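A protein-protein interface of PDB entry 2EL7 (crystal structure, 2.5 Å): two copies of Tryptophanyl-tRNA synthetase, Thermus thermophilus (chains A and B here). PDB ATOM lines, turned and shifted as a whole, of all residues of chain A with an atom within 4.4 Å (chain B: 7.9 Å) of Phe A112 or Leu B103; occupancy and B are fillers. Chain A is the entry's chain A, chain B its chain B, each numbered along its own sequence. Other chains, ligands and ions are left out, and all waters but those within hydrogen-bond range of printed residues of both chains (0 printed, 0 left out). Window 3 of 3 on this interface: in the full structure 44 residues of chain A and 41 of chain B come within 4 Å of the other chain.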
ATOM      1  N   LEU A 106      22.929  35.732   6.395  1.00  0.00           N
ATOM      2  CA  LEU A 106      21.889  35.437   7.377  1.00  0.00           C
ATOM      3  C   LEU A 106      22.504  35.008   8.697  1.00  0.00           C
ATOM      4  O   LEU A 106      22.115  35.499   9.755  1.00  0.00           O
ATOM      5  CB  LEU A 106      20.940  34.356   6.864  1.00  0.00           C
ATOM      6  CG  LEU A 106      20.079  34.799   5.689  1.00  0.00           C
ATOM      7  CD1 LEU A 106      19.356  33.622   5.105  1.00  0.00           C
ATOM      8  CD2 LEU A 106      19.119  35.854   6.153  1.00  0.00           C
ATOM      9  N   THR A 107      23.474  34.109   8.644  1.00  0.00           N
ATOM     10  CA  THR A 107      24.107  33.653   9.873  1.00  0.00           C
ATOM     11  C   THR A 107      24.743  34.815  10.655  1.00  0.00           C
ATOM     12  O   THR A 107      24.887  34.742  11.879  1.00  0.00           O
ATOM     13  CB  THR A 107      25.140  32.537   9.573  1.00  0.00           C
ATOM     14  OG1 THR A 107      26.155  33.028   8.696  1.00  0.00           O
ATOM     15  CG2 THR A 107      24.462  31.375   8.866  1.00  0.00           C
ATOM     16  N   MET A 109      23.394  37.962  10.819  1.00  0.00           N
ATOM     17  CA  MET A 109      22.431  38.978  11.236  1.00  0.00           C
ATOM     18  C   MET A 109      22.509  38.981  12.750  1.00  0.00           C
ATOM     19  O   MET A 109      22.546  37.920  13.382  1.00  0.00           O
ATOM     20  CB  MET A 109      21.010  38.627  10.801  1.00  0.00           C
ATOM     21  CG  MET A 109      20.828  38.561   9.281  1.00  0.00           C
ATOM     22  SD  MET A 109      20.740  40.147   8.450  1.00  0.00           S
ATOM     23  CE  MET A 109      19.152  40.798   9.129  1.00  0.00           C
ATOM     24  N   THR A 110      22.551  40.177  13.320  1.00  0.00           N
ATOM     25  CA  THR A 110      22.649  40.339  14.743  1.00  0.00           C
ATOM     26  C   THR A 110      21.625  39.558  15.550  1.00  0.00           C
ATOM     27  O   THR A 110      21.978  38.949  16.552  1.00  0.00           O
ATOM     28  CB  THR A 110      22.519  41.805  15.130  1.00  0.00           C
ATOM     29  OG1 THR A 110      23.461  42.568  14.384  1.00  0.00           O
ATOM     30  CG2 THR A 110      22.788  41.995  16.618  1.00  0.00           C
ATOM     31  N   GLN A 111      20.364  39.564  15.128  1.00  0.00           N
ATOM     32  CA  GLN A 111      19.347  38.876  15.910  1.00  0.00           C
ATOM     33  C   GLN A 111      19.588  37.396  15.979  1.00  0.00           C
ATOM     34  O   GLN A 111      19.617  36.824  17.066  1.00  0.00           O
ATOM     35  CB  GLN A 111      17.932  39.176  15.388  1.00  0.00           C
ATOM     36  CG  GLN A 111      17.431  40.548  15.825  1.00  0.00           C
ATOM     37  CD  GLN A 111      15.908  40.607  16.029  1.00  0.00           C
ATOM     38  OE1 GLN A 111      15.304  39.696  16.617  1.00  0.00           O
ATOM     39  NE2 GLN A 111      15.291  41.688  15.570  1.00  0.00           N
ATOM     40  N   PHE A 112      19.772  36.769  14.825  1.00  0.00           N
ATOM     41  CA  PHE A 112      20.031  35.337  14.789  1.00  0.00           C
ATOM     42  C   PHE A 112      21.256  34.966  15.621  1.00  0.00           C
ATOM     43  O   PHE A 112      21.228  34.001  16.383  1.00  0.00           O
ATOM     44  CB  PHE A 112      20.262  34.863  13.355  1.00  0.00           C
ATOM     45  CG  PHE A 112      20.862  33.489  13.274  1.00  0.00           C
ATOM     46  CD1 PHE A 112      20.071  32.354  13.469  1.00  0.00           C
ATOM     47  CD2 PHE A 112      22.217  33.328  13.025  1.00  0.00           C
ATOM     48  CE1 PHE A 112      20.623  31.086  13.413  1.00  0.00           C
ATOM     49  CE2 PHE A 112      22.793  32.047  12.965  1.00  0.00           C
ATOM     50  CZ  PHE A 112      21.996  30.926  13.159  1.00  0.00           C
ATOM     51  N   LYS A 113      22.323  35.745  15.462  1.00  0.00           N
ATOM     52  CA  LYS A 113      23.591  35.524  16.143  1.00  0.00           C
ATOM     53  C   LYS A 113      23.499  35.541  17.662  1.00  0.00           C
ATOM     54  O   LYS A 113      24.096  34.701  18.332  1.00  0.00           O
ATOM     55  CB  LYS A 113      24.602  36.574  15.679  1.00  0.00           C
ATOM     56  CG  LYS A 113      25.995  36.394  16.263  1.00  0.00           C
ATOM     57  CD  LYS A 113      26.612  37.729  16.579  1.00  0.00           C
ATOM     58  CE  LYS A 113      26.136  38.248  17.901  1.00  0.00           C
ATOM     59  NZ  LYS A 113      26.534  39.658  18.156  1.00  0.00           N
ATOM     60  N   ASP A 114      22.770  36.509  18.207  1.00  0.00           N
ATOM     61  CA  ASP A 114      22.618  36.611  19.657  1.00  0.00           C
ATOM     62  C   ASP A 114      21.827  35.447  20.234  1.00  0.00           C
ATOM     63  O   ASP A 114      22.126  34.975  21.328  1.00  0.00           O
ATOM     64  CB  ASP A 114      21.921  37.913  20.058  1.00  0.00           C
ATOM     65  CG  ASP A 114      22.812  39.140  19.890  1.00  0.00           C
ATOM     66  OD1 ASP A 114      24.050  39.000  19.946  1.00  0.00           O
ATOM     67  OD2 ASP A 114      22.275  40.257  19.727  1.00  0.00           O
ATOM     68  N   LYS A 115      20.808  34.986  19.516  1.00  0.00           N
ATOM     69  CA  LYS A 115      20.005  33.878  20.010  1.00  0.00           C
ATOM     70  C   LYS A 115      20.822  32.609  19.863  1.00  0.00           C
ATOM     71  O   LYS A 115      20.785  31.724  20.718  1.00  0.00           O
ATOM     72  CB  LYS A 115      18.683  33.779  19.231  1.00  0.00           C
ATOM     73  CG  LYS A 115      18.373  32.394  18.648  1.00  0.00           C
ATOM     74  CD  LYS A 115      17.882  31.388  19.695  1.00  0.00           C
ATOM     75  CE  LYS A 115      16.549  31.827  20.271  1.00  0.00           C
ATOM     76  NZ  LYS A 115      16.069  30.872  21.290  1.00  0.00           N
ATOM     77  N   ALA A 116      21.577  32.530  18.778  1.00  0.00           N
ATOM     78  CA  ALA A 116      22.404  31.358  18.518  1.00  0.00           C
ATOM     79  C   ALA A 116      23.531  31.225  19.540  1.00  0.00           C
ATOM     80  O   ALA A 116      24.208  30.200  19.593  1.00  0.00           O
ATOM     81  CB  ALA A 116      22.984  31.423  17.096  1.00  0.00           C
ATOM     82  N   VAL A 122      18.362  26.401  17.960  1.00  0.00           N
ATOM     83  CA  VAL A 122      18.489  27.359  16.888  1.00  0.00           C
ATOM     84  C   VAL A 122      17.637  26.875  15.720  1.00  0.00           C
ATOM     85  O   VAL A 122      18.080  26.089  14.883  1.00  0.00           O
ATOM     86  CB  VAL A 122      20.011  27.637  16.506  1.00  0.00           C
ATOM     87  CG1 VAL A 122      20.844  26.408  16.697  1.00  0.00           C
ATOM     88  CG2 VAL A 122      20.128  28.146  15.069  1.00  0.00           C
ATOM     89  N   SER A 124      15.476  27.017  12.217  1.00  0.00           N
ATOM     90  CA  SER A 124      15.726  27.601  10.899  1.00  0.00           C
ATOM     91  C   SER A 124      14.827  28.829  10.762  1.00  0.00           C
ATOM     92  O   SER A 124      15.119  29.744  10.003  1.00  0.00           O
ATOM     93  CB  SER A 124      15.430  26.579   9.790  1.00  0.00           C
ATOM     94  OG  SER A 124      16.200  25.414   9.982  1.00  0.00           O
ATOM     95  N   LEU A 126      14.367  31.129  13.015  1.00  0.00           N
ATOM     96  CA  LEU A 126      15.136  32.291  13.470  1.00  0.00           C
ATOM     97  C   LEU A 126      16.063  32.752  12.328  1.00  0.00           C
ATOM     98  O   LEU A 126      16.110  33.948  11.997  1.00  0.00           O
ATOM     99  CB  LEU A 126      16.020  31.963  14.700  1.00  0.00           C
ATOM    100  CG  LEU A 126      15.481  31.693  16.119  1.00  0.00           C
ATOM    101  CD1 LEU A 126      14.033  32.213  16.248  1.00  0.00           C
ATOM    102  CD2 LEU A 126      15.576  30.176  16.444  1.00  0.00           C
ATOM    103  N   LEU A 127      16.795  31.806  11.728  1.00  0.00           N
ATOM    104  CA  LEU A 127      17.717  32.161  10.653  1.00  0.00           C
ATOM    105  C   LEU A 127      17.036  32.765   9.419  1.00  0.00           C
ATOM    106  O   LEU A 127      17.477  33.794   8.908  1.00  0.00           O
ATOM    107  CB  LEU A 127      18.546  30.944  10.206  1.00  0.00           C
ATOM    108  CG  LEU A 127      19.508  31.222   9.029  1.00  0.00           C
ATOM    109  CD1 LEU A 127      20.697  32.022   9.537  1.00  0.00           C
ATOM    110  CD2 LEU A 127      20.001  29.920   8.406  1.00  0.00           C
ATOM    111  N   THR B  98       9.755  25.333   8.229  1.00  0.00           N
ATOM    112  CA  THR B  98      11.050  25.956   8.472  1.00  0.00           C
ATOM    113  C   THR B  98      11.129  26.302   9.969  1.00  0.00           C
ATOM    114  O   THR B  98      12.167  26.082  10.623  1.00  0.00           O
ATOM    115  CB  THR B  98      11.217  27.226   7.613  1.00  0.00           C
ATOM    116  OG1 THR B  98      11.312  26.862   6.229  1.00  0.00           O
ATOM    117  CG2 THR B  98      12.406  27.994   8.019  1.00  0.00           C
ATOM    118  N   LEU B 100       9.840  24.740  12.304  1.00  0.00           N
ATOM    119  CA  LEU B 100       9.937  23.513  13.093  1.00  0.00           C
ATOM    120  C   LEU B 100      11.188  22.680  12.832  1.00  0.00           C
ATOM    121  O   LEU B 100      11.276  21.562  13.309  1.00  0.00           O
ATOM    122  CB  LEU B 100       8.716  22.621  12.839  1.00  0.00           C
ATOM    123  CG  LEU B 100       7.272  23.141  13.035  1.00  0.00           C
ATOM    124  CD1 LEU B 100       6.309  22.009  12.783  1.00  0.00           C
ATOM    125  CD2 LEU B 100       7.065  23.689  14.438  1.00  0.00           C
ATOM    126  N   THR B 101      12.160  23.224  12.112  1.00  0.00           N
ATOM    127  CA  THR B 101      13.364  22.482  11.769  1.00  0.00           C
ATOM    128  C   THR B 101      14.663  23.003  12.396  1.00  0.00           C
ATOM    129  O   THR B 101      15.079  24.136  12.153  1.00  0.00           O
ATOM    130  CB  THR B 101      13.540  22.451  10.222  1.00  0.00           C
ATOM    131  OG1 THR B 101      12.336  21.946   9.615  1.00  0.00           O
ATOM    132  CG2 THR B 101      14.730  21.572   9.823  1.00  0.00           C
ATOM    133  N   PRO B 102      15.315  22.186  13.229  1.00  0.00           N
ATOM    134  CA  PRO B 102      16.567  22.674  13.835  1.00  0.00           C
ATOM    135  C   PRO B 102      17.637  22.898  12.762  1.00  0.00           C
ATOM    136  O   PRO B 102      17.882  22.011  11.935  1.00  0.00           O
ATOM    137  CB  PRO B 102      16.951  21.544  14.806  1.00  0.00           C
ATOM    138  CG  PRO B 102      15.593  20.961  15.209  1.00  0.00           C
ATOM    139  CD  PRO B 102      14.824  20.954  13.888  1.00  0.00           C
ATOM    140  N   LEU B 103      18.291  24.060  12.783  1.00  0.00           N
ATOM    141  CA  LEU B 103      19.326  24.372  11.788  1.00  0.00           C
ATOM    142  C   LEU B 103      20.318  23.204  11.577  1.00  0.00           C
ATOM    143  O   LEU B 103      20.636  22.840  10.432  1.00  0.00           O
ATOM    144  CB  LEU B 103      20.079  25.669  12.166  1.00  0.00           C
ATOM    145  CG  LEU B 103      21.181  26.132  11.179  1.00  0.00           C
ATOM    146  CD1 LEU B 103      20.597  26.195   9.747  1.00  0.00           C
ATOM    147  CD2 LEU B 103      21.747  27.498  11.567  1.00  0.00           C
ATOM    148  N   GLY B 104      20.798  22.617  12.672  1.00  0.00           N
ATOM    149  CA  GLY B 104      21.713  21.496  12.566  1.00  0.00           C
ATOM    150  C   GLY B 104      21.231  20.330  11.704  1.00  0.00           C
ATOM    151  O   GLY B 104      22.045  19.617  11.126  1.00  0.00           O
ATOM    152  N   ASP B 105      19.924  20.108  11.613  1.00  0.00           N
ATOM    153  CA  ASP B 105      19.409  19.019  10.782  1.00  0.00           C
ATOM    154  C   ASP B 105      19.624  19.294   9.303  1.00  0.00           C
ATOM    155  O   ASP B 105      19.666  18.381   8.492  1.00  0.00           O
ATOM    156  CB  ASP B 105      17.913  18.856  10.987  1.00  0.00           C
ATOM    157  CG  ASP B 105      17.582  18.103  12.219  1.00  0.00           C
ATOM    158  OD1 ASP B 105      16.420  18.216  12.646  1.00  0.00           O
ATOM    159  OD2 ASP B 105      18.467  17.394  12.750  1.00  0.00           O
ATOM    160  N   LEU B 106      19.703  20.572   8.952  1.00  0.00           N
ATOM    161  CA  LEU B 106      19.892  20.980   7.572  1.00  0.00           C
ATOM    162  C   LEU B 106      21.365  21.054   7.200  1.00  0.00           C
ATOM    163  O   LEU B 106      21.731  20.618   6.119  1.00  0.00           O
ATOM    164  CB  LEU B 106      19.203  22.333   7.322  1.00  0.00           C
ATOM    165  CG  LEU B 106      17.665  22.271   7.324  1.00  0.00           C
ATOM    166  CD1 LEU B 106      17.070  23.675   7.114  1.00  0.00           C
ATOM    167  CD2 LEU B 106      17.190  21.302   6.226  1.00  0.00           C
ATOM    168  N   THR B 107      22.208  21.573   8.094  1.00  0.00           N
ATOM    169  CA  THR B 107      23.640  21.708   7.799  1.00  0.00           C
ATOM    170  C   THR B 107      24.429  20.401   7.726  1.00  0.00           C
ATOM    171  O   THR B 107      25.516  20.357   7.137  1.00  0.00           O
ATOM    172  CB  THR B 107      24.352  22.615   8.813  1.00  0.00           C
ATOM    173  OG1 THR B 107      24.195  22.074  10.132  1.00  0.00           O
ATOM    174  CG2 THR B 107      23.781  24.035   8.755  1.00  0.00           C
ATOM    175  N   ARG B 108      23.887  19.348   8.320  1.00  0.00           N
ATOM    176  CA  ARG B 108      24.540  18.053   8.310  1.00  0.00           C
ATOM    177  C   ARG B 108      24.114  17.206   7.115  1.00  0.00           C
ATOM    178  O   ARG B 108      24.778  16.222   6.792  1.00  0.00           O
ATOM    179  CB  ARG B 108      24.244  17.311   9.614  1.00  0.00           C
ATOM    180  CG  ARG B 108      24.614  18.140  10.822  1.00  0.00           C
ATOM    181  CD  ARG B 108      24.244  17.479  12.141  1.00  0.00           C
ATOM    182  NE  ARG B 108      24.262  18.461  13.223  1.00  0.00           N
ATOM    183  CZ  ARG B 108      24.438  18.164  14.509  1.00  0.00           C
ATOM    184  NH1 ARG B 108      24.434  19.130  15.420  1.00  0.00           N
ATOM    185  NH2 ARG B 108      24.632  16.903  14.882  1.00  0.00           N
ATOM    186  N   MET B 109      23.014  17.579   6.458  1.00  0.00           N
ATOM    187  CA  MET B 109      22.553  16.820   5.286  1.00  0.00           C
ATOM    188  C   MET B 109      23.757  16.585   4.384  1.00  0.00           C
ATOM    189  O   MET B 109      24.553  17.507   4.141  1.00  0.00           O
ATOM    190  CB  MET B 109      21.490  17.601   4.508  1.00  0.00           C
ATOM    191  CG  MET B 109      20.225  17.910   5.284  1.00  0.00           C
ATOM    192  SD  MET B 109      19.210  16.459   5.561  1.00  0.00           S
ATOM    193  CE  MET B 109      18.649  16.131   3.888  1.00  0.00           C
ATOM    194  N   PHE B 112      24.029  18.923   1.227  1.00  0.00           N
ATOM    195  CA  PHE B 112      24.406  20.312   1.495  1.00  0.00           C
ATOM    196  C   PHE B 112      25.916  20.414   1.699  1.00  0.00           C
ATOM    197  O   PHE B 112      26.564  21.240   1.068  1.00  0.00           O
ATOM    198  CB  PHE B 112      23.682  20.856   2.737  1.00  0.00           C
ATOM    199  CG  PHE B 112      24.206  22.192   3.202  1.00  0.00           C
ATOM    200  CD1 PHE B 112      24.032  23.328   2.430  1.00  0.00           C
ATOM    201  CD2 PHE B 112      24.922  22.301   4.396  1.00  0.00           C
ATOM    202  CE1 PHE B 112      24.566  24.555   2.834  1.00  0.00           C
ATOM    203  CE2 PHE B 112      25.460  23.525   4.806  1.00  0.00           C
ATOM    204  CZ  PHE B 112      25.284  24.652   4.025  1.00  0.00           C
ATOM    205  N   LEU B 127      20.692  25.149   1.350  1.00  0.00           N
ATOM    206  CA  LEU B 127      20.430  24.643   2.691  1.00  0.00           C
ATOM    207  C   LEU B 127      18.972  24.249   2.934  1.00  0.00           C
ATOM    208  O   LEU B 127      18.684  23.161   3.445  1.00  0.00           O
ATOM    209  CB  LEU B 127      20.812  25.698   3.718  1.00  0.00           C
ATOM    210  CG  LEU B 127      20.558  25.317   5.185  1.00  0.00           C
ATOM    211  CD1 LEU B 127      21.575  24.261   5.624  1.00  0.00           C
ATOM    212  CD2 LEU B 127      20.679  26.539   6.059  1.00  0.00           C
ATOM    213  N   MET B 128      18.066  25.157   2.563  1.00  0.00           N
ATOM    214  CA  MET B 128      16.635  24.994   2.768  1.00  0.00           C
ATOM    215  C   MET B 128      15.841  24.131   1.796  1.00  0.00           C
ATOM    216  O   MET B 128      14.678  23.857   2.075  1.00  0.00           O
ATOM    217  CB  MET B 128      15.949  26.364   2.790  1.00  0.00           C
ATOM    218  CG  MET B 128      16.518  27.389   3.758  1.00  0.00           C
ATOM    219  SD  MET B 128      16.660  26.809   5.460  1.00  0.00           S
ATOM    220  CE  MET B 128      14.973  26.362   5.822  1.00  0.00           C
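Phe A112 touches one residue of chain B. Printed residues of chain A within 4 Å of Leu B103: Phe A112 (3.8 Å), Val A122 (2.9 Å) and Ser A124 (3.7 Å). Of the printed residues of chain A, Thr B98 touches Ser A124. Of the printed residues of chain B, Ser A124 touches Thr B98 (3.4 Å), Thr B101 (2.8 Å), Leu B103 (3.7 Å) and Leu B106 (3.5 Å). Of the printed residues of chain A, Thr B101 touches Ser A124. Of the printed residues of chain A, Leu B106 touches Ser A124. Leu B100 touches none of the printed residues of chain A. Phe B112 touches none of the printed residues of chain A.
Phe A112 touches Leu B103. Val A122 touches Pro B102. Ser A124 touches Thr B98 (CB to O, 3.4 Å). Ser A124 touches Leu B103 (OG to N, 3.7 Å). CD1 of Leu B106 touches OG of Ser A124 (3.5 Å).
Of the 14 printed residues of chain A, 3 touch a printed residue of chain B. Printed residues of chain A that touch a printed residue of chain B: Phe A112, Val A122 and Ser A124. Hydrophobic or aromatic side chains of chain A that line the printed part of chain B: Phe A112 and Val A122. Along chain B the printed residues that touch a printed residue of chain A span positions 98 to 106. Among the printed residues, 7 pairs touch across the chains. Among the printed residues, no Asp or Glu carboxylate lies within 4 Å of a Lys or Arg side-chain nitrogen of the other chain.
The side-chain hydroxyl (OG) of Ser A124 sits at hydrogen-bond distance from the backbone carbonyl oxygen (O) of Thr B101, at 2.8 Å. The backbone carbonyl oxygen of Val A122 sits at hydrogen-bond distance from the backbone NH of Leu B103.
5 positions are printed for both chains.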
